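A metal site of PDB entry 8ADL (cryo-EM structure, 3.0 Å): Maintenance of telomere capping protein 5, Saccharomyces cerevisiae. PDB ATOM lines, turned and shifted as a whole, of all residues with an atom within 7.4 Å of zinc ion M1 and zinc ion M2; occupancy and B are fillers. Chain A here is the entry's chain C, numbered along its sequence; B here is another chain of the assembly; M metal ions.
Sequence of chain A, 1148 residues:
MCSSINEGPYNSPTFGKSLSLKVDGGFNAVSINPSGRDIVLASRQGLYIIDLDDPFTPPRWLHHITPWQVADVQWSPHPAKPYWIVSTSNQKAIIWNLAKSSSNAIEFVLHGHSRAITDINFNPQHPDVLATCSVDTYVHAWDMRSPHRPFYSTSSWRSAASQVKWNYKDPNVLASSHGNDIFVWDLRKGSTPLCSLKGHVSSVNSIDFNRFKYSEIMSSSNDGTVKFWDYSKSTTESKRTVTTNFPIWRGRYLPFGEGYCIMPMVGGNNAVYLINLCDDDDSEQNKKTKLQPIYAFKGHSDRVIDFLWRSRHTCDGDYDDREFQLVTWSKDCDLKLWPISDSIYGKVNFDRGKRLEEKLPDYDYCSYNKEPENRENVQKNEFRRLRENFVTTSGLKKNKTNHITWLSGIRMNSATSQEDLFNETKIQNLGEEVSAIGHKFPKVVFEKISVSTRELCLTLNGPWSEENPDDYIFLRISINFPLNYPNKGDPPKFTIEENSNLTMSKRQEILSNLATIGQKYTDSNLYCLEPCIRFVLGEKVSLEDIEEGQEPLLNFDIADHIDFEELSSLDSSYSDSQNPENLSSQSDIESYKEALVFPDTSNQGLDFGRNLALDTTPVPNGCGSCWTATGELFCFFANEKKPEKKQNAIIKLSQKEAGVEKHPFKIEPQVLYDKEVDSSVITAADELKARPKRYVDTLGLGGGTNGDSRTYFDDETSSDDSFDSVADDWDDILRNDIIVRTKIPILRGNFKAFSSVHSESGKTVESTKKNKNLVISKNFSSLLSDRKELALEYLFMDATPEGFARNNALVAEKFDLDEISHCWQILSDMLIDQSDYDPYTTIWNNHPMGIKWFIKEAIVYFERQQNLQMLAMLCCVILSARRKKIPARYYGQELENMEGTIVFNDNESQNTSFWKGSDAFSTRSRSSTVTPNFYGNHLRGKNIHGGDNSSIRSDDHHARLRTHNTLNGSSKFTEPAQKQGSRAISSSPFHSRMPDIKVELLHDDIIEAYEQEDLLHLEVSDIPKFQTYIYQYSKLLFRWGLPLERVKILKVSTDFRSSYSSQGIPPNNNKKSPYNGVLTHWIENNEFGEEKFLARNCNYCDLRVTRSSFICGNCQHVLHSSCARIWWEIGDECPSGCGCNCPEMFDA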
ATOM      1  N   ASN A1099      12.813   2.411  29.736  1.00  0.00           N
ATOM      2  CA  ASN A1099      13.535   2.337  30.996  1.00  0.00           C
ATOM      3  C   ASN A1099      13.652   3.679  31.708  1.00  0.00           C
ATOM      4  O   ASN A1099      14.282   3.759  32.762  1.00  0.00           O
ATOM      5  CB  ASN A1099      14.932   1.758  30.761  1.00  0.00           C
ATOM      6  CG  ASN A1099      14.887   0.281  30.419  1.00  0.00           C
ATOM      7  OD1 ASN A1099      14.806  -0.566  31.307  1.00  0.00           O
ATOM      8  ND2 ASN A1099      14.925  -0.026  29.129  1.00  0.00           N
ATOM      9  N   PHE A1110      15.636   4.095  21.171  1.00  0.00           N
ATOM     10  CA  PHE A1110      17.085   4.080  21.259  1.00  0.00           C
ATOM     11  C   PHE A1110      17.528   2.757  21.886  1.00  0.00           C
ATOM     12  O   PHE A1110      17.042   2.386  22.953  1.00  0.00           O
ATOM     13  CB  PHE A1110      17.598   5.259  22.098  1.00  0.00           C
ATOM     14  CG  PHE A1110      18.970   5.057  22.677  1.00  0.00           C
ATOM     15  CD1 PHE A1110      20.091   5.002  21.863  1.00  0.00           C
ATOM     16  CD2 PHE A1110      19.140   4.929  24.046  1.00  0.00           C
ATOM     17  CE1 PHE A1110      21.355   4.814  22.400  1.00  0.00           C
ATOM     18  CE2 PHE A1110      20.397   4.747  24.587  1.00  0.00           C
ATOM     19  CZ  PHE A1110      21.508   4.690  23.756  1.00  0.00           C
ATOM     20  N   ILE A1111      18.434   2.055  21.211  1.00  0.00           N
ATOM     21  CA  ILE A1111      18.887   0.741  21.642  1.00  0.00           C
ATOM     22  C   ILE A1111      20.383   0.790  21.883  1.00  0.00           C
ATOM     23  O   ILE A1111      21.150   1.231  21.013  1.00  0.00           O
ATOM     24  CB  ILE A1111      18.537  -0.342  20.599  1.00  0.00           C
ATOM     25  CG1 ILE A1111      17.053  -0.282  20.233  1.00  0.00           C
ATOM     26  CG2 ILE A1111      18.909  -1.721  21.121  1.00  0.00           C
ATOM     27  CD1 ILE A1111      16.722  -0.946  18.925  1.00  0.00           C
ATOM     28  N   CYS A1112      20.811   0.328  23.057  1.00  0.00           N
ATOM     29  CA  CYS A1112      22.201   0.089  23.368  1.00  0.00           C
ATOM     30  C   CYS A1112      22.606  -1.321  22.966  1.00  0.00           C
ATOM     31  O   CYS A1112      21.771  -2.227  22.840  1.00  0.00           O
ATOM     32  CB  CYS A1112      22.460   0.303  24.861  1.00  0.00           C
ATOM     33  SG  CYS A1112      24.176   0.036  25.364  1.00  0.00           S
ATOM     34  N   GLY A1113      23.904  -1.511  22.764  1.00  0.00           N
ATOM     35  CA  GLY A1113      24.405  -2.804  22.327  1.00  0.00           C
ATOM     36  C   GLY A1113      24.920  -3.680  23.453  1.00  0.00           C
ATOM     37  O   GLY A1113      24.672  -4.895  23.457  1.00  0.00           O
ATOM     38  N   ASN A1114      25.644  -3.090  24.409  1.00  0.00           N
ATOM     39  CA  ASN A1114      26.164  -3.849  25.533  1.00  0.00           C
ATOM     40  C   ASN A1114      25.034  -4.342  26.431  1.00  0.00           C
ATOM     41  O   ASN A1114      24.961  -5.531  26.772  1.00  0.00           O
ATOM     42  CB  ASN A1114      27.163  -3.010  26.330  1.00  0.00           C
ATOM     43  CG  ASN A1114      28.124  -3.855  27.132  1.00  0.00           C
ATOM     44  OD1 ASN A1114      28.101  -5.083  27.069  1.00  0.00           O
ATOM     45  ND2 ASN A1114      28.987  -3.198  27.902  1.00  0.00           N
ATOM     46  N   CYS A1115      24.147  -3.438  26.839  1.00  0.00           N
ATOM     47  CA  CYS A1115      22.908  -3.803  27.508  1.00  0.00           C
ATOM     48  C   CYS A1115      21.750  -3.655  26.520  1.00  0.00           C
ATOM     49  O   CYS A1115      21.723  -2.718  25.712  1.00  0.00           O
ATOM     50  CB  CYS A1115      22.673  -2.944  28.757  1.00  0.00           C
ATOM     51  SG  CYS A1115      22.122  -1.251  28.478  1.00  0.00           S
ATOM     52  N   GLN A1116      20.825  -4.601  26.560  1.00  0.00           N
ATOM     53  CA  GLN A1116      19.753  -4.652  25.575  1.00  0.00           C
ATOM     54  C   GLN A1116      18.486  -4.033  26.151  1.00  0.00           C
ATOM     55  O   GLN A1116      17.506  -4.698  26.480  1.00  0.00           O
ATOM     56  CB  GLN A1116      19.535  -6.090  25.112  1.00  0.00           C
ATOM     57  CG  GLN A1116      20.708  -6.626  24.302  1.00  0.00           C
ATOM     58  CD  GLN A1116      20.672  -8.135  24.123  1.00  0.00           C
ATOM     59  OE1 GLN A1116      19.649  -8.778  24.393  1.00  0.00           O
ATOM     60  NE2 GLN A1116      21.778  -8.707  23.688  1.00  0.00           N
ATOM     61  N   HIS A1117      18.524  -2.703  26.277  1.00  0.00           N
ATOM     62  CA  HIS A1117      17.469  -1.931  26.907  1.00  0.00           C
ATOM     63  C   HIS A1117      16.995  -0.814  25.979  1.00  0.00           C
ATOM     64  O   HIS A1117      17.808  -0.140  25.352  1.00  0.00           O
ATOM     65  CB  HIS A1117      17.926  -1.334  28.239  1.00  0.00           C
ATOM     66  CG  HIS A1117      18.181  -2.353  29.305  1.00  0.00           C
ATOM     67  ND1 HIS A1117      19.183  -2.215  30.241  1.00  0.00           N
ATOM     68  CD2 HIS A1117      17.570  -3.528  29.587  1.00  0.00           C
ATOM     69  CE1 HIS A1117      19.181  -3.259  31.043  1.00  0.00           C
ATOM     70  NE2 HIS A1117      18.204  -4.072  30.677  1.00  0.00           N
ATOM     71  N   VAL A1118      15.673  -0.628  25.913  1.00  0.00           N
ATOM     72  CA  VAL A1118      15.073   0.393  25.060  1.00  0.00           C
ATOM     73  C   VAL A1118      14.985   1.716  25.818  1.00  0.00           C
ATOM     74  O   VAL A1118      15.002   1.755  27.053  1.00  0.00           O
ATOM     75  CB  VAL A1118      13.687  -0.034  24.565  1.00  0.00           C
ATOM     76  CG1 VAL A1118      13.796  -1.178  23.600  1.00  0.00           C
ATOM     77  CG2 VAL A1118      12.805  -0.410  25.735  1.00  0.00           C
ATOM     78  N   TRP A1128      20.256  11.638  28.777  1.00  0.00           N
ATOM     79  CA  TRP A1128      21.693  11.742  28.531  1.00  0.00           C
ATOM     80  C   TRP A1128      22.211  13.158  28.623  1.00  0.00           C
ATOM     81  O   TRP A1128      23.426  13.366  28.526  1.00  0.00           O
ATOM     82  CB  TRP A1128      22.057  11.132  27.178  1.00  0.00           C
ATOM     83  CG  TRP A1128      21.682   9.677  27.025  1.00  0.00           C
ATOM     84  CD1 TRP A1128      20.945   9.130  26.013  1.00  0.00           C
ATOM     85  CD2 TRP A1128      22.039   8.595  27.892  1.00  0.00           C
ATOM     86  NE1 TRP A1128      20.810   7.781  26.208  1.00  0.00           N
ATOM     87  CE2 TRP A1128      21.472   7.423  27.345  1.00  0.00           C
ATOM     88  CE3 TRP A1128      22.778   8.491  29.074  1.00  0.00           C
ATOM     89  CZ2 TRP A1128      21.620   6.180  27.945  1.00  0.00           C
ATOM     90  CZ3 TRP A1128      22.918   7.262  29.665  1.00  0.00           C
ATOM     91  CH2 TRP A1128      22.344   6.125  29.108  1.00  0.00           C
ATOM     92  N   GLU A1133      24.828   6.509  33.150  1.00  0.00           N
ATOM     93  CA  GLU A1133      24.624   5.069  33.043  1.00  0.00           C
ATOM     94  C   GLU A1133      23.212   4.787  32.550  1.00  0.00           C
ATOM     95  O   GLU A1133      22.411   5.711  32.337  1.00  0.00           O
ATOM     96  CB  GLU A1133      24.866   4.378  34.389  1.00  0.00           C
ATOM     97  CG  GLU A1133      26.289   4.523  34.913  1.00  0.00           C
ATOM     98  CD  GLU A1133      26.503   3.763  36.202  1.00  0.00           C
ATOM     99  OE1 GLU A1133      25.522   3.228  36.753  1.00  0.00           O
ATOM    100  OE2 GLU A1133      27.671   3.687  36.657  1.00  0.00           O
ATOM    101  N   CYS A1134      22.904   3.515  32.372  1.00  0.00           N
ATOM    102  CA  CYS A1134      21.569   3.110  31.938  1.00  0.00           C
ATOM    103  C   CYS A1134      20.550   3.432  33.028  1.00  0.00           C
ATOM    104  O   CYS A1134      20.816   3.187  34.208  1.00  0.00           O
ATOM    105  CB  CYS A1134      21.556   1.619  31.601  1.00  0.00           C
ATOM    106  SG  CYS A1134      20.036   1.012  30.829  1.00  0.00           S
ATOM    107  N   PRO A1135      19.392   3.999  32.669  1.00  0.00           N
ATOM    108  CA  PRO A1135      18.396   4.342  33.696  1.00  0.00           C
ATOM    109  C   PRO A1135      17.772   3.142  34.389  1.00  0.00           C
ATOM    110  O   PRO A1135      17.164   3.324  35.452  1.00  0.00           O
ATOM    111  CB  PRO A1135      17.341   5.130  32.899  1.00  0.00           C
ATOM    112  CG  PRO A1135      17.531   4.708  31.493  1.00  0.00           C
ATOM    113  CD  PRO A1135      18.989   4.451  31.328  1.00  0.00           C
ATOM    114  N   SER A1136      17.898   1.936  33.843  1.00  0.00           N
ATOM    115  CA  SER A1136      17.469   0.735  34.547  1.00  0.00           C
ATOM    116  C   SER A1136      18.461   0.294  35.607  1.00  0.00           C
ATOM    117  O   SER A1136      18.167  -0.647  36.354  1.00  0.00           O
ATOM    118  CB  SER A1136      17.233  -0.398  33.556  1.00  0.00           C
ATOM    119  OG  SER A1136      18.345  -0.591  32.715  1.00  0.00           O
ATOM    120  N   GLY A1137      19.630   0.935  35.683  1.00  0.00           N
ATOM    121  CA  GLY A1137      20.628   0.621  36.680  1.00  0.00           C
ATOM    122  C   GLY A1137      21.292  -0.733  36.502  1.00  0.00           C
ATOM    123  O   GLY A1137      21.511  -1.438  37.498  1.00  0.00           O
ATOM    124  N   CYS A1138      21.619  -1.102  35.277  1.00  0.00           N
ATOM    125  CA  CYS A1138      22.377  -2.323  35.016  1.00  0.00           C
ATOM    126  C   CYS A1138      23.880  -2.113  35.048  1.00  0.00           C
ATOM    127  O   CYS A1138      24.633  -3.079  34.929  1.00  0.00           O
ATOM    128  CB  CYS A1138      21.963  -2.924  33.669  1.00  0.00           C
ATOM    129  SG  CYS A1138      22.176  -1.811  32.260  1.00  0.00           S
ATOM    130  N   GLY A1139      24.336  -0.865  35.207  1.00  0.00           N
ATOM    131  CA  GLY A1139      25.756  -0.602  35.262  1.00  0.00           C
ATOM    132  C   GLY A1139      26.439  -0.460  33.920  1.00  0.00           C
ATOM    133  O   GLY A1139      27.670  -0.546  33.855  1.00  0.00           O
ATOM    134  N   CYS A1140      25.693  -0.246  32.849  1.00  0.00           N
ATOM    135  CA  CYS A1140      26.237  -0.142  31.502  1.00  0.00           C
ATOM    136  C   CYS A1140      26.392   1.327  31.129  1.00  0.00           C
ATOM    137  O   CYS A1140      25.411   2.073  31.128  1.00  0.00           O
ATOM    138  CB  CYS A1140      25.349  -0.861  30.495  1.00  0.00           C
ATOM    139  SG  CYS A1140      25.843  -0.587  28.773  1.00  0.00           S
ATOM    140  N   ASN A1141      27.619   1.735  30.805  1.00  0.00           N
ATOM    141  CA  ASN A1141      27.900   3.089  30.343  1.00  0.00           C
ATOM    142  C   ASN A1141      27.500   3.184  28.871  1.00  0.00           C
ATOM    143  O   ASN A1141      28.314   3.043  27.959  1.00  0.00           O
ATOM    144  CB  ASN A1141      29.366   3.444  30.560  1.00  0.00           C
ATOM    145  CG  ASN A1141      29.858   3.061  31.945  1.00  0.00           C
ATOM    146  OD1 ASN A1141      29.423   3.631  32.945  1.00  0.00           O
ATOM    147  ND2 ASN A1141      30.772   2.095  31.999  1.00  0.00           N
ATOM    148  N   CYS A1142      26.205   3.419  28.665  1.00  0.00           N
ATOM    149  CA  CYS A1142      25.640   3.450  27.325  1.00  0.00           C
ATOM    150  C   CYS A1142      26.183   4.526  26.376  1.00  0.00           C
ATOM    151  O   CYS A1142      26.185   4.258  25.164  1.00  0.00           O
ATOM    152  CB  CYS A1142      24.108   3.599  27.427  1.00  0.00           C
ATOM    153  SG  CYS A1142      23.259   2.203  28.150  1.00  0.00           S
ATOM    154  N   PRO A1143      26.635   5.712  26.815  1.00  0.00           N
ATOM    155  CA  PRO A1143      27.346   6.593  25.865  1.00  0.00           C
ATOM    156  C   PRO A1143      28.651   6.034  25.306  1.00  0.00           C
ATOM    157  O   PRO A1143      29.109   6.528  24.268  1.00  0.00           O
ATOM    158  CB  PRO A1143      27.604   7.852  26.699  1.00  0.00           C
ATOM    159  CG  PRO A1143      26.439   7.931  27.573  1.00  0.00           C
ATOM    160  CD  PRO A1143      26.149   6.505  27.966  1.00  0.00           C
ATOM    161  N   MET A1145      29.208   2.386  25.166  1.00  0.00           N
ATOM    162  CA  MET A1145      29.088   0.963  24.888  1.00  0.00           C
ATOM    163  C   MET A1145      27.822   0.638  24.097  1.00  0.00           C
ATOM    164  O   MET A1145      27.325  -0.490  24.174  1.00  0.00           O
ATOM    165  CB  MET A1145      29.105   0.152  26.184  1.00  0.00           C
ATOM    166  CG  MET A1145      30.491  -0.111  26.749  1.00  0.00           C
ATOM    167  SD  MET A1145      31.350  -1.440  25.894  1.00  0.00           S
ATOM    168  CE  MET A1145      32.843  -0.597  25.362  1.00  0.00           C
ATOM    169  N   PHE A1146      27.290   1.591  23.338  1.00  0.00           N
ATOM    170  CA  PHE A1146      26.098   1.333  22.542  1.00  0.00           C
ATOM    171  C   PHE A1146      26.408   0.764  21.160  1.00  0.00           C
ATOM    172  O   PHE A1146      25.477   0.556  20.375  1.00  0.00           O
ATOM    173  CB  PHE A1146      25.242   2.597  22.412  1.00  0.00           C
ATOM    174  CG  PHE A1146      25.840   3.668  21.547  1.00  0.00           C
ATOM    175  CD1 PHE A1146      26.799   4.530  22.037  1.00  0.00           C
ATOM    176  CD2 PHE A1146      25.401   3.842  20.244  1.00  0.00           C
ATOM    177  CE1 PHE A1146      27.339   5.527  21.239  1.00  0.00           C
ATOM    178  CE2 PHE A1146      25.943   4.832  19.434  1.00  0.00           C
ATOM    179  CZ  PHE A1146      26.906   5.673  19.935  1.00  0.00           C
ATOM    180  N   ILE B 872      18.035  -6.200  38.184  1.00  0.00           N
ATOM    181  CA  ILE B 872      17.956  -5.377  36.983  1.00  0.00           C
ATOM    182  C   ILE B 872      16.937  -5.974  36.020  1.00  0.00           C
ATOM    183  O   ILE B 872      16.557  -7.149  36.101  1.00  0.00           O
ATOM    184  CB  ILE B 872      19.330  -5.243  36.301  1.00  0.00           C
ATOM    185  CG1 ILE B 872      19.836  -6.606  35.820  1.00  0.00           C
ATOM    186  CG2 ILE B 872      20.329  -4.613  37.260  1.00  0.00           C
ATOM    187  CD1 ILE B 872      21.047  -6.536  34.926  1.00  0.00           C
ATOM    188  N   LYS B 873      16.489  -5.134  35.092  1.00  0.00           N
ATOM    189  CA  LYS B 873      15.537  -5.563  34.070  1.00  0.00           C
ATOM    190  C   LYS B 873      16.223  -6.498  33.082  1.00  0.00           C
ATOM    191  O   LYS B 873      17.372  -6.257  32.693  1.00  0.00           O
ATOM    192  CB  LYS B 873      14.943  -4.357  33.349  1.00  0.00           C
ATOM    193  CG  LYS B 873      13.731  -4.667  32.488  1.00  0.00           C
ATOM    194  CD  LYS B 873      13.199  -3.434  31.795  1.00  0.00           C
ATOM    195  CE  LYS B 873      12.181  -2.706  32.654  1.00  0.00           C
ATOM    196  NZ  LYS B 873      10.844  -3.363  32.589  1.00  0.00           N
ATOM    197  N   GLN B 876      15.875  -6.832  26.543  1.00  0.00           N
ATOM    198  CA  GLN B 876      14.594  -6.584  25.868  1.00  0.00           C
ATOM    199  C   GLN B 876      14.656  -6.777  24.365  1.00  0.00           C
ATOM    200  O   GLN B 876      13.909  -7.591  23.822  1.00  0.00           O
ATOM    201  CB  GLN B 876      14.114  -5.167  26.198  1.00  0.00           C
ATOM    202  CG  GLN B 876      13.973  -4.882  27.682  1.00  0.00           C
ATOM    203  CD  GLN B 876      13.546  -3.450  27.965  1.00  0.00           C
ATOM    204  OE1 GLN B 876      14.337  -2.516  27.844  1.00  0.00           O
ATOM    205  NE2 GLN B 876      12.291  -3.287  28.356  1.00  0.00           N
HETATM  206 ZN    ZN M   1      20.915  -1.098  30.454  1.00  0.00          ZN
HETATM  207 ZN    ZN M   2      23.897   0.028  27.669  1.00  0.00          ZN
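The side-chain hydroxyl of Ser 1136 sits close to a ring nitrogen (ND1) of His 1117 (3.1 Å). O of Lys 873 of chain B sits at hydrogen-bond distance from NE2 of His 1117 (3.1 Å). N of Cys 1134 is in hydrogen-bond range of O of Cys 1140. The side-chain hydroxyl of Ser 1136 lies close to the side-chain sulfur of Cys 1134 (3.0 Å). The side-chain sulfur of Cys 1112 sits close to the backbone NH of Asn 1114, 3.6 Å away. The backbone carbonyl oxygen of Met 1145 sits close to the side-chain sulfur of Cys 1112 (3.4 Å).
Merely in contact with zinc ion M1: Ser 1136. Five residues have an atom within 4 Å of zinc ion M1: Cys 1115, His 1117, Cys 1134, Ser 1136 and Cys 1138. Along chain A the residues within 4 Å of zinc ion M1 span positions 1115 to 1138.
The nearest printed residue that does not touch zinc ion M2 is Asn 1114 (4.7 Å).
Zinc ion M1 is bound by ND1 of His 1117 (2.1 Å), SG of Cys 1138 (2.3 Å), SG of Cys 1134 (2.3 Å) and SG of Cys 1115 (2.3 Å). Zinc ion M1 has four donor atoms within binding distance.
Zinc ion M2 is bound by the side-chain sulfur (SG) of Cys 1142 (2.3 Å). SG of Cys 1140 is bound to zinc ion M2, at 2.3 Å. SG of Cys 1112 binds zinc ion M2. SG of Cys 1115 is bound to zinc ion M2 (2.3 Å). Zinc ion M2 has four donor atoms within binding distance.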
